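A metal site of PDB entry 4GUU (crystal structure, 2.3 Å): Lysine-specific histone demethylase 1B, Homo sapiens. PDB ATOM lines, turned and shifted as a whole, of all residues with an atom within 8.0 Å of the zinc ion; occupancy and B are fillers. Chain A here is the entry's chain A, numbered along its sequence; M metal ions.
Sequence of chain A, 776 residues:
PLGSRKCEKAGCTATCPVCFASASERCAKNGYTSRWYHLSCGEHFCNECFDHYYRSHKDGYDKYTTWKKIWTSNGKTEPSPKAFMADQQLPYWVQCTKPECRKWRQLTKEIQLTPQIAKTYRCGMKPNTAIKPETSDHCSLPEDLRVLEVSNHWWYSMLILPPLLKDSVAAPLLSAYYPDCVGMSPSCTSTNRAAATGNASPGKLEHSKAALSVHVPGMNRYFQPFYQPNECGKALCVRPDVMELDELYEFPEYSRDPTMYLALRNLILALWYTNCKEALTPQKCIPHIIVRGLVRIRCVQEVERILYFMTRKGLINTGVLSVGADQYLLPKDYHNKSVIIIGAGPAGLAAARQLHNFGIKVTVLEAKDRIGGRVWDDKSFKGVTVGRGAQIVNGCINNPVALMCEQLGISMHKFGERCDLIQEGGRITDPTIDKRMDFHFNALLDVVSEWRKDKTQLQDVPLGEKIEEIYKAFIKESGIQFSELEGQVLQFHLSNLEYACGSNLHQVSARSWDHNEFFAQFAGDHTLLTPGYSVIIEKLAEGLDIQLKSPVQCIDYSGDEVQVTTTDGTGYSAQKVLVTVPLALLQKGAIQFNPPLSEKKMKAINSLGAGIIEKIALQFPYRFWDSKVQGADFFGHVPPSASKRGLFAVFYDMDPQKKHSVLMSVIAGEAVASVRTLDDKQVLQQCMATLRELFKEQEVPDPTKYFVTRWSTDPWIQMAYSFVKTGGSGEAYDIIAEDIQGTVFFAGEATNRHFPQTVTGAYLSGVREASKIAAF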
ATOM      1  N   VAL A  18     -19.420  21.583  26.947  1.00  0.00           N
ATOM      2  CA  VAL A  18     -19.460  22.934  26.401  1.00  0.00           C
ATOM      3  C   VAL A  18     -19.037  23.885  27.508  1.00  0.00           C
ATOM      4  O   VAL A  18     -19.168  23.562  28.691  1.00  0.00           O
ATOM      5  CB  VAL A  18     -20.870  23.301  25.902  1.00  0.00           C
ATOM      6  CG1 VAL A  18     -21.321  22.335  24.827  1.00  0.00           C
ATOM      7  CG2 VAL A  18     -21.859  23.337  27.058  1.00  0.00           C
ATOM      8  N   CYS A  19     -18.508  25.039  27.141  1.00  0.00           N
ATOM      9  CA  CYS A  19     -18.029  25.974  28.164  1.00  0.00           C
ATOM     10  C   CYS A  19     -19.102  26.948  28.646  1.00  0.00           C
ATOM     11  O   CYS A  19     -19.674  27.693  27.852  1.00  0.00           O
ATOM     12  CB  CYS A  19     -16.807  26.740  27.663  1.00  0.00           C
ATOM     13  SG  CYS A  19     -16.197  27.892  28.899  1.00  0.00           S
ATOM     14  N   PHE A  20     -19.350  26.946  29.955  1.00  0.00           N
ATOM     15  CA  PHE A  20     -20.358  27.819  30.542  1.00  0.00           C
ATOM     16  C   PHE A  20     -19.828  29.227  30.755  1.00  0.00           C
ATOM     17  O   PHE A  20     -20.598  30.175  30.916  1.00  0.00           O
ATOM     18  CB  PHE A  20     -20.868  27.239  31.872  1.00  0.00           C
ATOM     19  CG  PHE A  20     -19.812  27.146  32.949  1.00  0.00           C
ATOM     20  CD1 PHE A  20     -19.296  25.909  33.318  1.00  0.00           C
ATOM     21  CD2 PHE A  20     -19.357  28.274  33.603  1.00  0.00           C
ATOM     22  CE1 PHE A  20     -18.334  25.812  34.305  1.00  0.00           C
ATOM     23  CE2 PHE A  20     -18.391  28.179  34.598  1.00  0.00           C
ATOM     24  CZ  PHE A  20     -17.877  26.947  34.943  1.00  0.00           C
ATOM     25  N   ALA A  21     -18.504  29.356  30.761  1.00  0.00           N
ATOM     26  CA  ALA A  21     -17.864  30.623  31.102  1.00  0.00           C
ATOM     27  C   ALA A  21     -17.874  31.650  29.970  1.00  0.00           C
ATOM     28  O   ALA A  21     -18.281  32.795  30.164  1.00  0.00           O
ATOM     29  CB  ALA A  21     -16.441  30.376  31.579  1.00  0.00           C
ATOM     30  N   SER A  22     -17.403  31.235  28.793  1.00  0.00           N
ATOM     31  CA  SER A  22     -17.217  32.152  27.672  1.00  0.00           C
ATOM     32  C   SER A  22     -16.670  33.481  28.174  1.00  0.00           C
ATOM     33  O   SER A  22     -17.163  34.555  27.810  1.00  0.00           O
ATOM     34  CB  SER A  22     -18.518  32.357  26.894  1.00  0.00           C
ATOM     35  OG  SER A  22     -19.471  33.058  27.672  1.00  0.00           O
ATOM     36  N   ALA A  23     -15.641  33.405  29.011  1.00  0.00           N
ATOM     37  CA  ALA A  23     -15.065  34.597  29.613  1.00  0.00           C
ATOM     38  C   ALA A  23     -13.949  35.138  28.734  1.00  0.00           C
ATOM     39  O   ALA A  23     -13.722  36.354  28.667  1.00  0.00           O
ATOM     40  CB  ALA A  23     -14.548  34.292  31.005  1.00  0.00           C
ATOM     41  N   SER A  24     -13.235  34.239  28.068  1.00  0.00           N
ATOM     42  CA  SER A  24     -12.139  34.635  27.199  1.00  0.00           C
ATOM     43  C   SER A  24     -12.619  34.832  25.775  1.00  0.00           C
ATOM     44  O   SER A  24     -13.475  34.084  25.288  1.00  0.00           O
ATOM     45  CB  SER A  24     -11.024  33.583  27.240  1.00  0.00           C
ATOM     46  OG  SER A  24     -10.082  33.789  26.197  1.00  0.00           O
ATOM     47  N   GLU A  25     -12.099  35.853  25.100  1.00  0.00           N
ATOM     48  CA  GLU A  25     -12.442  36.098  23.716  1.00  0.00           C
ATOM     49  C   GLU A  25     -11.979  34.931  22.847  1.00  0.00           C
ATOM     50  O   GLU A  25     -12.389  34.801  21.692  1.00  0.00           O
ATOM     51  CB  GLU A  25     -11.800  37.398  23.217  1.00  0.00           C
ATOM     52  CG  GLU A  25     -10.282  37.358  23.124  1.00  0.00           C
ATOM     53  CD  GLU A  25      -9.589  37.446  24.470  1.00  0.00           C
ATOM     54  OE1 GLU A  25     -10.231  37.864  25.455  1.00  0.00           O
ATOM     55  OE2 GLU A  25      -8.390  37.087  24.536  1.00  0.00           O
ATOM     56  N   ARG A  26     -11.136  34.081  23.432  1.00  0.00           N
ATOM     57  CA  ARG A  26     -10.598  32.927  22.743  1.00  0.00           C
ATOM     58  C   ARG A  26     -11.203  31.634  23.291  1.00  0.00           C
ATOM     59  O   ARG A  26     -10.653  30.546  23.131  1.00  0.00           O
ATOM     60  CB  ARG A  26      -9.076  32.893  22.871  1.00  0.00           C
ATOM     61  CG  ARG A  26      -8.410  34.251  22.707  1.00  0.00           C
ATOM     62  CD  ARG A  26      -6.902  34.124  22.684  1.00  0.00           C
ATOM     63  NE  ARG A  26      -6.470  33.174  21.667  1.00  0.00           N
ATOM     64  CZ  ARG A  26      -5.284  33.196  21.083  1.00  0.00           C
ATOM     65  NH1 ARG A  26      -4.403  34.142  21.397  1.00  0.00           N
ATOM     66  NH2 ARG A  26      -4.977  32.288  20.168  1.00  0.00           N
ATOM     67  N   CYS A  27     -12.354  31.782  23.954  1.00  0.00           N
ATOM     68  CA  CYS A  27     -13.089  30.652  24.508  1.00  0.00           C
ATOM     69  C   CYS A  27     -13.334  29.547  23.484  1.00  0.00           C
ATOM     70  O   CYS A  27     -13.730  29.796  22.340  1.00  0.00           O
ATOM     71  CB  CYS A  27     -14.411  31.145  25.094  1.00  0.00           C
ATOM     72  SG  CYS A  27     -15.553  29.832  25.574  1.00  0.00           S
ATOM     73  N   ALA A  28     -13.118  28.310  23.910  1.00  0.00           N
ATOM     74  CA  ALA A  28     -13.308  27.150  23.051  1.00  0.00           C
ATOM     75  C   ALA A  28     -14.772  26.890  22.726  1.00  0.00           C
ATOM     76  O   ALA A  28     -15.085  26.103  21.838  1.00  0.00           O
ATOM     77  CB  ALA A  28     -12.690  25.914  23.695  1.00  0.00           C
ATOM     78  N   LYS A  29     -15.674  27.512  23.455  1.00  0.00           N
ATOM     79  CA  LYS A  29     -17.112  27.306  23.323  1.00  0.00           C
ATOM     80  C   LYS A  29     -17.406  25.830  23.382  1.00  0.00           C
ATOM     81  O   LYS A  29     -17.085  25.185  24.316  1.00  0.00           O
ATOM     82  CB  LYS A  29     -17.683  27.907  22.054  1.00  0.00           C
ATOM     83  CG  LYS A  29     -17.050  29.181  21.663  1.00  0.00           C
ATOM     84  CD  LYS A  29     -17.967  30.333  21.837  1.00  0.00           C
ATOM     85  CE  LYS A  29     -17.485  31.527  21.044  1.00  0.00           C
ATOM     86  NZ  LYS A  29     -18.128  31.622  19.742  1.00  0.00           N
ATOM     87  N   ASN A  30     -18.043  25.324  22.366  1.00  0.00           N
ATOM     88  CA  ASN A  30     -18.343  23.905  22.326  1.00  0.00           C
ATOM     89  C   ASN A  30     -17.383  23.043  21.525  1.00  0.00           C
ATOM     90  O   ASN A  30     -17.615  21.851  21.328  1.00  0.00           O
ATOM     91  CB  ASN A  30     -19.761  23.752  21.787  1.00  0.00           C
ATOM     92  CG  ASN A  30     -19.903  24.282  20.366  1.00  0.00           C
ATOM     93  OD1 ASN A  30     -20.900  23.997  19.688  1.00  0.00           O
ATOM     94  ND2 ASN A  30     -18.921  25.039  19.905  1.00  0.00           N
ATOM     95  N   THR A  33     -10.608  22.088  22.935  1.00  0.00           N
ATOM     96  CA  THR A  33      -9.759  22.842  23.850  1.00  0.00           C
ATOM     97  C   THR A  33      -8.643  21.967  24.413  1.00  0.00           C
ATOM     98  O   THR A  33      -8.769  20.742  24.477  1.00  0.00           O
ATOM     99  CB  THR A  33     -10.545  23.427  25.025  1.00  0.00           C
ATOM    100  OG1 THR A  33      -9.698  24.297  25.785  1.00  0.00           O
ATOM    101  CG2 THR A  33     -11.053  22.312  25.936  1.00  0.00           C
ATOM    102  N   TRP A  36     -10.559  20.316  29.204  1.00  0.00           N
ATOM    103  CA  TRP A  36     -11.882  20.668  29.729  1.00  0.00           C
ATOM    104  C   TRP A  36     -11.916  20.512  31.231  1.00  0.00           C
ATOM    105  O   TRP A  36     -11.575  19.451  31.756  1.00  0.00           O
ATOM    106  CB  TRP A  36     -12.957  19.793  29.095  1.00  0.00           C
ATOM    107  CG  TRP A  36     -13.407  20.240  27.738  1.00  0.00           C
ATOM    108  CD1 TRP A  36     -13.149  19.622  26.554  1.00  0.00           C
ATOM    109  CD2 TRP A  36     -14.173  21.411  27.433  1.00  0.00           C
ATOM    110  NE1 TRP A  36     -13.715  20.336  25.519  1.00  0.00           N
ATOM    111  CE2 TRP A  36     -14.350  21.432  26.030  1.00  0.00           C
ATOM    112  CE3 TRP A  36     -14.725  22.440  28.206  1.00  0.00           C
ATOM    113  CZ2 TRP A  36     -15.061  22.450  25.390  1.00  0.00           C
ATOM    114  CZ3 TRP A  36     -15.426  23.447  27.563  1.00  0.00           C
ATOM    115  CH2 TRP A  36     -15.586  23.442  26.171  1.00  0.00           C
ATOM    116  N   HIS A  44     -18.843  22.435  32.622  1.00  0.00           N
ATOM    117  CA  HIS A  44     -17.413  22.487  32.322  1.00  0.00           C
ATOM    118  C   HIS A  44     -16.985  23.854  31.823  1.00  0.00           C
ATOM    119  O   HIS A  44     -17.816  24.646  31.368  1.00  0.00           O
ATOM    120  CB  HIS A  44     -17.058  21.446  31.270  1.00  0.00           C
ATOM    121  CG  HIS A  44     -17.430  20.042  31.644  1.00  0.00           C
ATOM    122  ND1 HIS A  44     -18.695  19.543  31.465  1.00  0.00           N
ATOM    123  CD2 HIS A  44     -16.693  19.043  32.182  1.00  0.00           C
ATOM    124  CE1 HIS A  44     -18.725  18.284  31.878  1.00  0.00           C
ATOM    125  NE2 HIS A  44     -17.530  17.958  32.315  1.00  0.00           N
ATOM    126  N   PHE A  45     -15.691  24.121  31.895  1.00  0.00           N
ATOM    127  CA  PHE A  45     -15.119  25.322  31.288  1.00  0.00           C
ATOM    128  C   PHE A  45     -13.760  25.010  30.660  1.00  0.00           C
ATOM    129  O   PHE A  45     -12.982  24.209  31.182  1.00  0.00           O
ATOM    130  CB  PHE A  45     -15.039  26.482  32.278  1.00  0.00           C
ATOM    131  CG  PHE A  45     -14.170  26.211  33.479  1.00  0.00           C
ATOM    132  CD1 PHE A  45     -12.940  26.808  33.609  1.00  0.00           C
ATOM    133  CD2 PHE A  45     -14.612  25.357  34.482  1.00  0.00           C
ATOM    134  CE1 PHE A  45     -12.143  26.577  34.718  1.00  0.00           C
ATOM    135  CE2 PHE A  45     -13.825  25.105  35.592  1.00  0.00           C
ATOM    136  CZ  PHE A  45     -12.579  25.711  35.710  1.00  0.00           C
ATOM    137  N   CYS A  46     -13.485  25.643  29.523  1.00  0.00           N
ATOM    138  CA  CYS A  46     -12.301  25.337  28.716  1.00  0.00           C
ATOM    139  C   CYS A  46     -11.029  25.973  29.260  1.00  0.00           C
ATOM    140  O   CYS A  46     -11.066  26.910  30.043  1.00  0.00           O
ATOM    141  CB  CYS A  46     -12.518  25.803  27.285  1.00  0.00           C
ATOM    142  SG  CYS A  46     -12.399  27.596  27.124  1.00  0.00           S
ATOM    143  N   ASN A  47      -9.898  25.465  28.784  1.00  0.00           N
ATOM    144  CA  ASN A  47      -8.587  25.887  29.283  1.00  0.00           C
ATOM    145  C   ASN A  47      -8.294  27.377  29.161  1.00  0.00           C
ATOM    146  O   ASN A  47      -7.670  27.951  30.044  1.00  0.00           O
ATOM    147  CB  ASN A  47      -7.472  25.069  28.620  1.00  0.00           C
ATOM    148  CG  ASN A  47      -6.104  25.374  29.208  1.00  0.00           C
ATOM    149  OD1 ASN A  47      -5.336  26.152  28.643  1.00  0.00           O
ATOM    150  ND2 ASN A  47      -5.796  24.770  30.349  1.00  0.00           N
ATOM    151  N   GLU A  48      -8.742  28.009  28.075  1.00  0.00           N
ATOM    152  CA  GLU A  48      -8.491  29.444  27.876  1.00  0.00           C
ATOM    153  C   GLU A  48      -9.328  30.342  28.799  1.00  0.00           C
ATOM    154  O   GLU A  48      -8.905  31.453  29.120  1.00  0.00           O
ATOM    155  CB  GLU A  48      -8.686  29.866  26.424  1.00  0.00           C
ATOM    156  CG  GLU A  48      -9.657  29.007  25.645  1.00  0.00           C
ATOM    157  CD  GLU A  48      -8.984  27.798  25.042  1.00  0.00           C
ATOM    158  OE1 GLU A  48      -9.575  26.704  25.103  1.00  0.00           O
ATOM    159  OE2 GLU A  48      -7.868  27.945  24.492  1.00  0.00           O
ATOM    160  N   CYS A  49     -10.508  29.888  29.199  1.00  0.00           N
ATOM    161  CA  CYS A  49     -11.279  30.623  30.186  1.00  0.00           C
ATOM    162  C   CYS A  49     -10.666  30.388  31.563  1.00  0.00           C
ATOM    163  O   CYS A  49     -10.666  31.264  32.416  1.00  0.00           O
ATOM    164  CB  CYS A  49     -12.765  30.236  30.140  1.00  0.00           C
ATOM    165  SG  CYS A  49     -13.661  30.902  28.707  1.00  0.00           S
ATOM    166  N   PHE A  50     -10.122  29.181  31.752  1.00  0.00           N
ATOM    167  CA  PHE A  50      -9.313  28.875  32.926  1.00  0.00           C
ATOM    168  C   PHE A  50      -8.179  29.891  33.032  1.00  0.00           C
ATOM    169  O   PHE A  50      -8.062  30.619  34.023  1.00  0.00           O
ATOM    170  CB  PHE A  50      -8.753  27.462  32.795  1.00  0.00           C
ATOM    171  CG  PHE A  50      -7.976  27.004  34.000  1.00  0.00           C
ATOM    172  CD1 PHE A  50      -8.552  26.145  34.924  1.00  0.00           C
ATOM    173  CD2 PHE A  50      -6.670  27.419  34.195  1.00  0.00           C
ATOM    174  CE1 PHE A  50      -7.833  25.715  36.021  1.00  0.00           C
ATOM    175  CE2 PHE A  50      -5.951  26.989  35.292  1.00  0.00           C
ATOM    176  CZ  PHE A  50      -6.532  26.137  36.205  1.00  0.00           C
ATOM    177  N   HIS A  52      -7.765  32.664  31.422  1.00  0.00           N
ATOM    178  CA  HIS A  52      -8.242  34.040  31.413  1.00  0.00           C
ATOM    179  C   HIS A  52      -8.243  34.623  32.824  1.00  0.00           C
ATOM    180  O   HIS A  52      -8.048  35.819  33.016  1.00  0.00           O
ATOM    181  CB  HIS A  52      -9.647  34.110  30.807  1.00  0.00           C
ATOM    182  CG  HIS A  52     -10.201  35.497  30.719  1.00  0.00           C
ATOM    183  ND1 HIS A  52     -10.929  36.082  31.708  1.00  0.00           N
ATOM    184  CD2 HIS A  52     -10.123  36.421  29.713  1.00  0.00           C
ATOM    185  CE1 HIS A  52     -11.294  37.306  31.344  1.00  0.00           C
ATOM    186  NE2 HIS A  52     -10.807  37.519  30.133  1.00  0.00           N
ATOM    187  N   MET A  85     -15.115  29.701  39.922  1.00  0.00           N
ATOM    188  CA  MET A  85     -16.108  29.506  38.868  1.00  0.00           C
ATOM    189  C   MET A  85     -17.469  29.137  39.435  1.00  0.00           C
ATOM    190  O   MET A  85     -18.502  29.554  38.915  1.00  0.00           O
ATOM    191  CB  MET A  85     -15.630  28.443  37.875  1.00  0.00           C
ATOM    192  CG  MET A  85     -14.486  28.876  36.968  1.00  0.00           C
ATOM    193  SD  MET A  85     -14.995  29.902  35.586  1.00  0.00           S
ATOM    194  CE  MET A  85     -14.570  31.534  36.187  1.00  0.00           C
HETATM  195 ZN    ZN M   1     -14.376  29.027  27.703  1.00  0.00          ZN
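The backbone NH (N) of Ser 22 lies close to the side-chain sulfur (SG) of Cys 49 (3.8 Å).
The side-chain sulfur (SG) of Cys 46 lies close to the backbone NH (N) of Ala 28 (3.4 Å).
SG of Cys 49 lies close to N of Ala 23 (3.2 Å).
The side-chain carboxylate (OE1) of Glu 48 lies close to the side-chain sulfur (SG) of Cys 46 (3.6 Å).
The side-chain sulfur (SG) of Cys 27 lies close to the backbone NH (N) of Lys 29, 3.1 Å away.
The side-chain sulfur of Cys 19 lies close to the backbone NH of Ser 22, 3.6 Å away.
O of Lys 29 lies within hydrogen-bond range of N of Cys 19 (3.2 Å).
N of Ala 21 lies close to SG of Cys 19 (3.3 Å).
Merely in contact with the zinc ion: Ser 22.
Of the 24 residues printed, 5 come within 4 Å of the zinc ion.
The zinc ion is bound by SG of Cys 49, SG of Cys 19, SG of Cys 46 and SG of Cys 27.
The zinc ion has four donor atoms within binding distance.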
